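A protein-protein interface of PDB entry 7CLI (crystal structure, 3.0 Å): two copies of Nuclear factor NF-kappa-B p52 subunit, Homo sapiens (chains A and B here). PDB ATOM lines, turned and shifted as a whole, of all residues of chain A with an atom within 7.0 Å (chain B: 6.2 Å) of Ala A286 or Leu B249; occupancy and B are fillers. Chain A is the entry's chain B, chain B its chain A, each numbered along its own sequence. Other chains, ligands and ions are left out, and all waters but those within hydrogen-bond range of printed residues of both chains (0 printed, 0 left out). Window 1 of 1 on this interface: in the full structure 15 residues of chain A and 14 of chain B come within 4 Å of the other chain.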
ATOM      1  N   TYR A 247     -11.023  -7.994  16.233  1.00  0.00           N
ATOM      2  CA  TYR A 247     -12.299  -7.416  15.766  1.00  0.00           C
ATOM      3  C   TYR A 247     -12.994  -6.936  17.036  1.00  0.00           C
ATOM      4  O   TYR A 247     -13.314  -7.727  17.943  1.00  0.00           O
ATOM      5  CB  TYR A 247     -13.191  -8.432  15.039  1.00  0.00           C
ATOM      6  CG  TYR A 247     -12.769  -8.778  13.635  1.00  0.00           C
ATOM      7  CD1 TYR A 247     -11.474  -9.192  13.369  1.00  0.00           C
ATOM      8  CD2 TYR A 247     -13.653  -8.702  12.569  1.00  0.00           C
ATOM      9  CE1 TYR A 247     -11.070  -9.534  12.091  1.00  0.00           C
ATOM     10  CE2 TYR A 247     -13.262  -9.041  11.283  1.00  0.00           C
ATOM     11  CZ  TYR A 247     -11.968  -9.465  11.049  1.00  0.00           C
ATOM     12  OH  TYR A 247     -11.517  -9.804   9.813  1.00  0.00           O
ATOM     13  N   LEU A 248     -13.231  -5.650  17.123  1.00  0.00           N
ATOM     14  CA  LEU A 248     -13.889  -5.067  18.308  1.00  0.00           C
ATOM     15  C   LEU A 248     -15.241  -4.536  17.876  1.00  0.00           C
ATOM     16  O   LEU A 248     -15.274  -3.740  16.978  1.00  0.00           O
ATOM     17  CB  LEU A 248     -12.949  -4.020  18.889  1.00  0.00           C
ATOM     18  CG  LEU A 248     -13.432  -3.353  20.161  1.00  0.00           C
ATOM     19  CD1 LEU A 248     -12.226  -2.848  20.940  1.00  0.00           C
ATOM     20  CD2 LEU A 248     -14.429  -2.232  19.826  1.00  0.00           C
ATOM     21  N   LEU A 249     -16.313  -4.939  18.555  1.00  0.00           N
ATOM     22  CA  LEU A 249     -17.675  -4.434  18.263  1.00  0.00           C
ATOM     23  C   LEU A 249     -17.951  -3.290  19.228  1.00  0.00           C
ATOM     24  O   LEU A 249     -17.715  -3.399  20.416  1.00  0.00           O
ATOM     25  CB  LEU A 249     -18.740  -5.528  18.417  1.00  0.00           C
ATOM     26  CG  LEU A 249     -18.463  -6.857  17.722  1.00  0.00           C
ATOM     27  CD1 LEU A 249     -19.752  -7.648  17.558  1.00  0.00           C
ATOM     28  CD2 LEU A 249     -17.790  -6.630  16.376  1.00  0.00           C
ATOM     29  N   CYS A 250     -18.408  -2.172  18.717  1.00  0.00           N
ATOM     30  CA  CYS A 250     -18.683  -1.005  19.598  1.00  0.00           C
ATOM     31  C   CYS A 250     -19.982  -0.282  19.251  1.00  0.00           C
ATOM     32  O   CYS A 250     -20.667  -0.692  18.320  1.00  0.00           O
ATOM     33  CB  CYS A 250     -17.484  -0.070  19.577  1.00  0.00           C
ATOM     34  SG  CYS A 250     -16.896   0.285  17.900  1.00  0.00           S
ATOM     35  N   ASP A 251     -20.307   0.768  20.002  1.00  0.00           N
ATOM     36  CA  ASP A 251     -21.431   1.660  19.683  1.00  0.00           C
ATOM     37  C   ASP A 251     -20.828   2.738  18.807  1.00  0.00           C
ATOM     38  O   ASP A 251     -19.603   2.667  18.481  1.00  0.00           O
ATOM     39  CB  ASP A 251     -22.171   2.157  20.923  1.00  0.00           C
ATOM     40  CG  ASP A 251     -23.041   1.070  21.539  1.00  0.00           C
ATOM     41  OD1 ASP A 251     -23.297   0.049  20.846  1.00  0.00           O
ATOM     42  OD2 ASP A 251     -23.437   1.233  22.713  1.00  0.00           O
ATOM     43  N   VAL A 253     -19.052   5.067  16.388  1.00  0.00           N
ATOM     44  CA  VAL A 253     -17.774   5.818  16.466  1.00  0.00           C
ATOM     45  C   VAL A 253     -17.438   6.456  15.129  1.00  0.00           C
ATOM     46  O   VAL A 253     -17.529   5.775  14.083  1.00  0.00           O
ATOM     47  CB  VAL A 253     -16.602   4.951  16.966  1.00  0.00           C
ATOM     48  CG1 VAL A 253     -16.795   4.551  18.419  1.00  0.00           C
ATOM     49  CG2 VAL A 253     -16.371   3.729  16.094  1.00  0.00           C
ATOM     50  N   ASP A 280     -10.461   0.810   8.264  1.00  0.00           N
ATOM     51  CA  ASP A 280     -10.575  -0.378   9.124  1.00  0.00           C
ATOM     52  C   ASP A 280     -11.739  -0.268  10.087  1.00  0.00           C
ATOM     53  O   ASP A 280     -12.021  -1.278  10.716  1.00  0.00           O
ATOM     54  CB  ASP A 280      -9.249  -0.735   9.807  1.00  0.00           C
ATOM     55  CG  ASP A 280      -8.319  -1.516   8.890  1.00  0.00           C
ATOM     56  OD1 ASP A 280      -8.299  -1.189   7.682  1.00  0.00           O
ATOM     57  OD2 ASP A 280      -7.651  -2.484   9.379  1.00  0.00           O
ATOM     58  N   VAL A 281     -12.292   0.935  10.232  1.00  0.00           N
ATOM     59  CA  VAL A 281     -13.456   1.176  11.085  1.00  0.00           C
ATOM     60  C   VAL A 281     -14.651   0.883  10.211  1.00  0.00           C
ATOM     61  O   VAL A 281     -14.933   1.659   9.265  1.00  0.00           O
ATOM     62  CB  VAL A 281     -13.497   2.619  11.620  1.00  0.00           C
ATOM     63  CG1 VAL A 281     -14.885   3.017  12.126  1.00  0.00           C
ATOM     64  CG2 VAL A 281     -12.429   2.848  12.681  1.00  0.00           C
ATOM     65  N   HIS A 282     -15.305  -0.220  10.500  1.00  0.00           N
ATOM     66  CA  HIS A 282     -16.440  -0.743   9.690  1.00  0.00           C
ATOM     67  C   HIS A 282     -17.806  -0.172  10.111  1.00  0.00           C
ATOM     68  O   HIS A 282     -18.329  -0.554  11.197  1.00  0.00           O
ATOM     69  CB  HIS A 282     -16.421  -2.276   9.708  1.00  0.00           C
ATOM     70  CG  HIS A 282     -17.595  -2.900   9.036  1.00  0.00           C
ATOM     71  ND1 HIS A 282     -17.690  -3.030   7.662  1.00  0.00           N
ATOM     72  CD2 HIS A 282     -18.737  -3.396   9.554  1.00  0.00           C
ATOM     73  CE1 HIS A 282     -18.837  -3.604   7.367  1.00  0.00           C
ATOM     74  NE2 HIS A 282     -19.490  -3.863   8.516  1.00  0.00           N
ATOM     75  N   LYS A 283     -18.428   0.600   9.199  1.00  0.00           N
ATOM     76  CA  LYS A 283     -19.799   1.134   9.322  1.00  0.00           C
ATOM     77  C   LYS A 283     -20.018   1.732  10.708  1.00  0.00           C
ATOM     78  O   LYS A 283     -21.141   1.601  11.221  1.00  0.00           O
ATOM     79  CB  LYS A 283     -20.767  -0.007   9.001  1.00  0.00           C
ATOM     80  CG  LYS A 283     -20.645  -0.561   7.585  1.00  0.00           C
ATOM     81  CD  LYS A 283     -21.112   0.408   6.501  1.00  0.00           C
ATOM     82  CE  LYS A 283     -21.042  -0.152   5.097  1.00  0.00           C
ATOM     83  NZ  LYS A 283     -22.384  -0.280   4.480  1.00  0.00           N
ATOM     84  N   GLN A 284     -18.955   2.321  11.270  1.00  0.00           N
ATOM     85  CA  GLN A 284     -18.903   3.006  12.593  1.00  0.00           C
ATOM     86  C   GLN A 284     -19.215   2.141  13.825  1.00  0.00           C
ATOM     87  O   GLN A 284     -19.293   2.669  14.923  1.00  0.00           O
ATOM     88  CB  GLN A 284     -19.834   4.223  12.542  1.00  0.00           C
ATOM     89  CG  GLN A 284     -19.604   5.105  11.322  1.00  0.00           C
ATOM     90  CD  GLN A 284     -20.148   6.499  11.512  1.00  0.00           C
ATOM     91  OE1 GLN A 284     -19.405   7.462  11.725  1.00  0.00           O
ATOM     92  NE2 GLN A 284     -21.464   6.611  11.450  1.00  0.00           N
ATOM     93  N   TYR A 285     -19.317   0.815  13.676  1.00  0.00           N
ATOM     94  CA  TYR A 285     -19.759  -0.067  14.773  1.00  0.00           C
ATOM     95  C   TYR A 285     -18.850  -1.284  15.010  1.00  0.00           C
ATOM     96  O   TYR A 285     -19.136  -2.240  15.778  1.00  0.00           O
ATOM     97  CB  TYR A 285     -21.226  -0.471  14.593  1.00  0.00           C
ATOM     98  CG  TYR A 285     -22.190   0.692  14.653  1.00  0.00           C
ATOM     99  CD1 TYR A 285     -22.555   1.297  15.851  1.00  0.00           C
ATOM    100  CD2 TYR A 285     -22.725   1.217  13.486  1.00  0.00           C
ATOM    101  CE1 TYR A 285     -23.425   2.374  15.887  1.00  0.00           C
ATOM    102  CE2 TYR A 285     -23.581   2.306  13.501  1.00  0.00           C
ATOM    103  CZ  TYR A 285     -23.936   2.882  14.707  1.00  0.00           C
ATOM    104  OH  TYR A 285     -24.793   3.943  14.704  1.00  0.00           O
ATOM    105  N   ALA A 286     -17.713  -1.313  14.347  1.00  0.00           N
ATOM    106  CA  ALA A 286     -16.672  -2.316  14.546  1.00  0.00           C
ATOM    107  C   ALA A 286     -15.358  -1.636  14.180  1.00  0.00           C
ATOM    108  O   ALA A 286     -15.291  -0.648  13.404  1.00  0.00           O
ATOM    109  CB  ALA A 286     -16.958  -3.534  13.701  1.00  0.00           C
ATOM    110  N   ILE A 287     -14.316  -2.161  14.770  1.00  0.00           N
ATOM    111  CA  ILE A 287     -12.929  -1.770  14.473  1.00  0.00           C
ATOM    112  C   ILE A 287     -12.108  -3.042  14.313  1.00  0.00           C
ATOM    113  O   ILE A 287     -12.087  -3.840  15.256  1.00  0.00           O
ATOM    114  CB  ILE A 287     -12.395  -0.879  15.593  1.00  0.00           C
ATOM    115  CG1 ILE A 287     -13.184   0.434  15.668  1.00  0.00           C
ATOM    116  CG2 ILE A 287     -10.887  -0.688  15.413  1.00  0.00           C
ATOM    117  CD1 ILE A 287     -12.473   1.547  16.421  1.00  0.00           C
ATOM    118  N   VAL A 288     -11.478  -3.237  13.156  1.00  0.00           N
ATOM    119  CA  VAL A 288     -10.429  -4.278  13.045  1.00  0.00           C
ATOM    120  C   VAL A 288      -9.095  -3.583  13.267  1.00  0.00           C
ATOM    121  O   VAL A 288      -8.780  -2.576  12.659  1.00  0.00           O
ATOM    122  CB  VAL A 288     -10.488  -5.113  11.763  1.00  0.00           C
ATOM    123  CG1 VAL A 288      -9.386  -6.158  11.767  1.00  0.00           C
ATOM    124  CG2 VAL A 288     -11.848  -5.780  11.622  1.00  0.00           C
ATOM    125  N   LYS B 229     -23.623  -7.728   1.311  1.00  0.00           N
ATOM    126  CA  LYS B 229     -22.153  -7.877   1.147  1.00  0.00           C
ATOM    127  C   LYS B 229     -21.480  -8.300   2.458  1.00  0.00           C
ATOM    128  O   LYS B 229     -21.767  -7.732   3.482  1.00  0.00           O
ATOM    129  CB  LYS B 229     -21.581  -6.549   0.641  1.00  0.00           C
ATOM    130  CG  LYS B 229     -20.073  -6.508   0.381  1.00  0.00           C
ATOM    131  CD  LYS B 229     -19.657  -6.906  -1.019  1.00  0.00           C
ATOM    132  CE  LYS B 229     -18.532  -6.036  -1.555  1.00  0.00           C
ATOM    133  NZ  LYS B 229     -18.002  -6.532  -2.847  1.00  0.00           N
ATOM    134  N   ILE B 230     -20.619  -9.300   2.364  1.00  0.00           N
ATOM    135  CA  ILE B 230     -19.776  -9.741   3.478  1.00  0.00           C
ATOM    136  C   ILE B 230     -18.475  -8.981   3.280  1.00  0.00           C
ATOM    137  O   ILE B 230     -17.788  -9.202   2.237  1.00  0.00           O
ATOM    138  CB  ILE B 230     -19.523 -11.247   3.501  1.00  0.00           C
ATOM    139  CG1 ILE B 230     -20.740 -12.023   3.984  1.00  0.00           C
ATOM    140  CG2 ILE B 230     -18.290 -11.551   4.343  1.00  0.00           C
ATOM    141  CD1 ILE B 230     -20.580 -13.522   3.829  1.00  0.00           C
ATOM    142  N   SER B 231     -18.184  -8.089   4.221  1.00  0.00           N
ATOM    143  CA  SER B 231     -17.002  -7.196   4.105  1.00  0.00           C
ATOM    144  C   SER B 231     -15.782  -7.951   4.569  1.00  0.00           C
ATOM    145  O   SER B 231     -14.840  -7.987   3.851  1.00  0.00           O
ATOM    146  CB  SER B 231     -17.180  -5.913   4.818  1.00  0.00           C
ATOM    147  OG  SER B 231     -18.050  -5.096   4.055  1.00  0.00           O
ATOM    148  N   ARG B 232     -15.854  -8.613   5.703  1.00  0.00           N
ATOM    149  CA  ARG B 232     -14.696  -9.203   6.350  1.00  0.00           C
ATOM    150  C   ARG B 232     -15.101 -10.267   7.364  1.00  0.00           C
ATOM    151  O   ARG B 232     -16.142 -10.078   8.012  1.00  0.00           O
ATOM    152  CB  ARG B 232     -14.059  -7.983   7.016  1.00  0.00           C
ATOM    153  CG  ARG B 232     -12.577  -8.082   7.266  1.00  0.00           C
ATOM    154  CD  ARG B 232     -12.135  -6.706   7.678  1.00  0.00           C
ATOM    155  NE  ARG B 232     -10.708  -6.674   7.927  1.00  0.00           N
ATOM    156  CZ  ARG B 232     -10.012  -5.553   8.097  1.00  0.00           C
ATOM    157  NH1 ARG B 232     -10.622  -4.379   8.037  1.00  0.00           N
ATOM    158  NH2 ARG B 232      -8.708  -5.605   8.326  1.00  0.00           N
ATOM    159  N   MET B 233     -14.307 -11.299   7.587  1.00  0.00           N
ATOM    160  CA  MET B 233     -14.605 -12.125   8.760  1.00  0.00           C
ATOM    161  C   MET B 233     -13.312 -12.532   9.405  1.00  0.00           C
ATOM    162  O   MET B 233     -12.367 -12.751   8.671  1.00  0.00           O
ATOM    163  CB  MET B 233     -15.425 -13.353   8.364  1.00  0.00           C
ATOM    164  CG  MET B 233     -14.727 -14.339   7.446  1.00  0.00           C
ATOM    165  SD  MET B 233     -15.903 -15.571   6.805  1.00  0.00           S
ATOM    166  CE  MET B 233     -17.228 -14.474   6.292  1.00  0.00           C
ATOM    167  N   TYR B 247     -16.661 -13.753  13.846  1.00  0.00           N
ATOM    168  CA  TYR B 247     -17.160 -12.368  13.788  1.00  0.00           C
ATOM    169  C   TYR B 247     -17.241 -12.037  12.305  1.00  0.00           C
ATOM    170  O   TYR B 247     -16.203 -12.018  11.619  1.00  0.00           O
ATOM    171  CB  TYR B 247     -16.214 -11.402  14.514  1.00  0.00           C
ATOM    172  CG  TYR B 247     -16.310 -11.424  16.018  1.00  0.00           C
ATOM    173  CD1 TYR B 247     -16.181 -12.616  16.708  1.00  0.00           C
ATOM    174  CD2 TYR B 247     -16.501 -10.260  16.751  1.00  0.00           C
ATOM    175  CE1 TYR B 247     -16.260 -12.657  18.087  1.00  0.00           C
ATOM    176  CE2 TYR B 247     -16.569 -10.282  18.135  1.00  0.00           C
ATOM    177  CZ  TYR B 247     -16.456 -11.491  18.802  1.00  0.00           C
ATOM    178  OH  TYR B 247     -16.540 -11.582  20.160  1.00  0.00           O
ATOM    179  N   LEU B 248     -18.426 -11.776  11.806  1.00  0.00           N
ATOM    180  CA  LEU B 248     -18.627 -11.458  10.382  1.00  0.00           C
ATOM    181  C   LEU B 248     -19.044 -10.001  10.281  1.00  0.00           C
ATOM    182  O   LEU B 248     -20.034  -9.663  10.890  1.00  0.00           O
ATOM    183  CB  LEU B 248     -19.683 -12.420   9.850  1.00  0.00           C
ATOM    184  CG  LEU B 248     -19.953 -12.311   8.358  1.00  0.00           C
ATOM    185  CD1 LEU B 248     -20.501 -13.634   7.833  1.00  0.00           C
ATOM    186  CD2 LEU B 248     -20.886 -11.131   8.066  1.00  0.00           C
ATOM    187  N   LEU B 249     -18.329  -9.193   9.488  1.00  0.00           N
ATOM    188  CA  LEU B 249     -18.690  -7.784   9.286  1.00  0.00           C
ATOM    189  C   LEU B 249     -19.475  -7.719   7.988  1.00  0.00           C
ATOM    190  O   LEU B 249     -19.066  -8.257   6.963  1.00  0.00           O
ATOM    191  CB  LEU B 249     -17.466  -6.865   9.243  1.00  0.00           C
ATOM    192  CG  LEU B 249     -16.529  -6.930  10.447  1.00  0.00           C
ATOM    193  CD1 LEU B 249     -15.736  -5.644  10.583  1.00  0.00           C
ATOM    194  CD2 LEU B 249     -17.278  -7.193  11.739  1.00  0.00           C
ATOM    195  N   CYS B 250     -20.597  -7.051   7.988  1.00  0.00           N
ATOM    196  CA  CYS B 250     -21.373  -6.914   6.725  1.00  0.00           C
ATOM    197  C   CYS B 250     -21.971  -5.525   6.520  1.00  0.00           C
ATOM    198  O   CYS B 250     -21.775  -4.672   7.358  1.00  0.00           O
ATOM    199  CB  CYS B 250     -22.458  -7.980   6.707  1.00  0.00           C
ATOM    200  SG  CYS B 250     -23.340  -8.116   8.277  1.00  0.00           S
ATOM    201  N   ASP B 251     -22.715  -5.311   5.455  1.00  0.00           N
ATOM    202  CA  ASP B 251     -23.473  -4.081   5.199  1.00  0.00           C
ATOM    203  C   ASP B 251     -24.794  -4.327   5.886  1.00  0.00           C
ATOM    204  O   ASP B 251     -24.991  -5.434   6.425  1.00  0.00           O
ATOM    205  CB  ASP B 251     -23.624  -3.793   3.703  1.00  0.00           C
ATOM    206  CG  ASP B 251     -22.333  -3.408   2.999  1.00  0.00           C
ATOM    207  OD1 ASP B 251     -21.346  -3.104   3.700  1.00  0.00           O
ATOM    208  OD2 ASP B 251     -22.330  -3.404   1.749  1.00  0.00           O
ATOM    209  N   HIS B 282     -25.118  -7.206  15.877  1.00  0.00           N
ATOM    210  CA  HIS B 282     -24.656  -5.895  16.406  1.00  0.00           C
ATOM    211  C   HIS B 282     -24.909  -4.740  15.424  1.00  0.00           C
ATOM    212  O   HIS B 282     -24.178  -4.665  14.370  1.00  0.00           O
ATOM    213  CB  HIS B 282     -23.171  -6.088  16.768  1.00  0.00           C
ATOM    214  CG  HIS B 282     -22.431  -4.876  17.217  1.00  0.00           C
ATOM    215  ND1 HIS B 282     -22.142  -4.656  18.546  1.00  0.00           N
ATOM    216  CD2 HIS B 282     -21.839  -3.877  16.529  1.00  0.00           C
ATOM    217  CE1 HIS B 282     -21.455  -3.541  18.665  1.00  0.00           C
ATOM    218  NE2 HIS B 282     -21.256  -3.048  17.442  1.00  0.00           N
ATOM    219  N   TYR B 285     -24.675  -4.425  11.435  1.00  0.00           N
ATOM    220  CA  TYR B 285     -23.442  -4.456  10.627  1.00  0.00           C
ATOM    221  C   TYR B 285     -22.474  -5.593  10.994  1.00  0.00           C
ATOM    222  O   TYR B 285     -21.276  -5.590  10.544  1.00  0.00           O
ATOM    223  CB  TYR B 285     -22.743  -3.097  10.697  1.00  0.00           C
ATOM    224  CG  TYR B 285     -23.495  -1.983  10.019  1.00  0.00           C
ATOM    225  CD1 TYR B 285     -23.534  -1.891   8.636  1.00  0.00           C
ATOM    226  CD2 TYR B 285     -24.170  -1.019  10.753  1.00  0.00           C
ATOM    227  CE1 TYR B 285     -24.200  -0.860   7.991  1.00  0.00           C
ATOM    228  CE2 TYR B 285     -24.849   0.016  10.127  1.00  0.00           C
ATOM    229  CZ  TYR B 285     -24.849   0.102   8.739  1.00  0.00           C
ATOM    230  OH  TYR B 285     -25.508   1.086   8.064  1.00  0.00           O
ATOM    231  N   ALA B 286     -22.882  -6.478  11.911  1.00  0.00           N
ATOM    232  CA  ALA B 286     -21.981  -7.543  12.347  1.00  0.00           C
ATOM    233  C   ALA B 286     -22.824  -8.726  12.772  1.00  0.00           C
ATOM    234  O   ALA B 286     -24.004  -8.596  13.056  1.00  0.00           O
ATOM    235  CB  ALA B 286     -21.058  -7.069  13.445  1.00  0.00           C
ATOM    236  N   ILE B 287     -22.214  -9.873  12.763  1.00  0.00           N
ATOM    237  CA  ILE B 287     -22.847 -11.110  13.277  1.00  0.00           C
ATOM    238  C   ILE B 287     -21.765 -11.888  13.996  1.00  0.00           C
ATOM    239  O   ILE B 287     -20.749 -12.213  13.377  1.00  0.00           O
ATOM    240  CB  ILE B 287     -23.463 -11.954  12.139  1.00  0.00           C
ATOM    241  CG1 ILE B 287     -24.662 -11.268  11.481  1.00  0.00           C
ATOM    242  CG2 ILE B 287     -23.823 -13.346  12.631  1.00  0.00           C
ATOM    243  CD1 ILE B 287     -24.807 -11.560   9.997  1.00  0.00           C
ATOM    244  N   LEU B 309     -24.448 -15.113   3.418  1.00  0.00           N
ATOM    245  CA  LEU B 309     -25.582 -14.518   4.133  1.00  0.00           C
ATOM    246  C   LEU B 309     -26.821 -14.698   3.267  1.00  0.00           C
ATOM    247  O   LEU B 309     -26.695 -14.630   2.065  1.00  0.00           O
ATOM    248  CB  LEU B 309     -25.409 -13.017   4.352  1.00  0.00           C
ATOM    249  CG  LEU B 309     -24.172 -12.551   5.097  1.00  0.00           C
ATOM    250  CD1 LEU B 309     -23.957 -11.070   4.806  1.00  0.00           C
ATOM    251  CD2 LEU B 309     -24.323 -12.816   6.589  1.00  0.00           C
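NE2 of His B282 sits at hydrogen-bond distance from O of Cys A250 (2.6 Å).
The side-chain carboxylate (OD1) of Asp B251 is in salt-bridge range of the side-chain amino group (NZ) of Lys A283, 3.1 Å away.
A ring nitrogen (NE2) of His A282 sits at hydrogen-bond distance from the backbone carbonyl oxygen (O) of Tyr B285, 3.2 Å away.
O of Cys B250 sits at hydrogen-bond distance from NE2 of His A282, at 2.7 Å.
OD2 of Asp A280 is in salt-bridge range of NH2 of Arg B232, at 3.5 Å.
The backbone carbonyl oxygen (O) of Tyr A285 sits at hydrogen-bond distance from a ring nitrogen (NE2) of His B282 (2.8 Å).
The backbone carbonyl oxygen (O) of Met B233 is in hydrogen-bond range of the side-chain hydroxyl (OH) of Tyr A247 (3.3 Å).
N of Val A288 is in hydrogen-bond range of O of Asp A280, at 3.2 Å.
The backbone NH of Cys B250 sits at hydrogen-bond distance from the backbone carbonyl oxygen of Tyr B285.
The backbone carbonyl oxygen (O) of Leu B249 sits at hydrogen-bond distance from the backbone NH (N) of Ser B231 (2.9 Å).
O of Arg B232 is in hydrogen-bond range of N of Leu B249 (2.8 Å).
The backbone NH (N) of Asp B251 is in hydrogen-bond range of the backbone carbonyl oxygen (O) of Lys B229, at 3.3 Å.
O of Tyr A285 sits at hydrogen-bond distance from N of Cys A250 (3.0 Å).
OH of Tyr A247 touches CG of Arg B232, at 3.3 Å.
Leu B249 touches Tyr A247.
Tyr B247 touches Leu A249 (CD2 to CD2, 3.9 Å).
Leu A249 touches His B282 (CB to CE1, 3.4 Å).
CE1 of His A282 touches OG of Ser B231, at 3.7 Å.
His A282 touches Leu B249.
Tyr B285 touches Lys A283.
CD2 of Tyr B285 touches CD2 of Tyr A285, at 3.8 Å.
Leu B249 touches Ala A286 (CD1 to CB, 3.96 Å).
Val A288 touches Arg B232 (CG1 to NH2, 3.6 Å).
Of the printed residues of chain B, Ala A286 touches Leu B249.
Of chain A, only Tyr A247 (3.98 Å), His A282 (3.5 Å) and Ala A286 (3.96 Å) come within 4 Å of Leu B249.
Of the printed residues of chain B, Val A288 touches Arg B232 (3.6 Å).
Of the printed residues of chain B, Leu A249 touches Tyr B247 and His B282.
Val A281 touches none of the printed residues of chain B.
The nearest printed residue of chain A that does not touch Ser B231 is Lys A283 (5.9 Å).
Of the 15 printed residues of chain B, 9 touch a printed residue of chain A.
Printed residues of chain A that touch a printed residue of chain B: Tyr A247, Leu A249, Cys A250, Asp A280, His A282, Lys A283, Tyr A285, Ala A286 and Val A288.
Hydrophobic or aromatic side chains of chain A that line the printed part of chain B: Tyr A247, Leu A249, His A282, Tyr A285, Ala A286 and Val A288.
Among the printed residues, 17 pairs touch across the chains.
Among the printed residues, Asp or Glu carboxylates within 4 Å of a Lys or Arg side-chain nitrogen of the other chain: Asp A280 with Arg B232 and Lys A283 with Asp B251.
Tyr A247 touches Leu B249, and with the chains exchanged Leu A249 touches Tyr B247.
Cys A250 touches His B282, and with the chains exchanged His A282 touches Cys B250.
Tyr A285 touches its own counterpart, Tyr B285.
Ala A286 touches Leu B249, but with the chains exchanged Leu A249 does not touch Ala B286 (4.4 Å).
Positions printed for both chains: 247, 248, 249, 250, 251, 282, 285, 286 and 287.
Of the 17 pairs that touch across the chains among the printed residues, 9 have their exchanged pair printed and touching as well.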
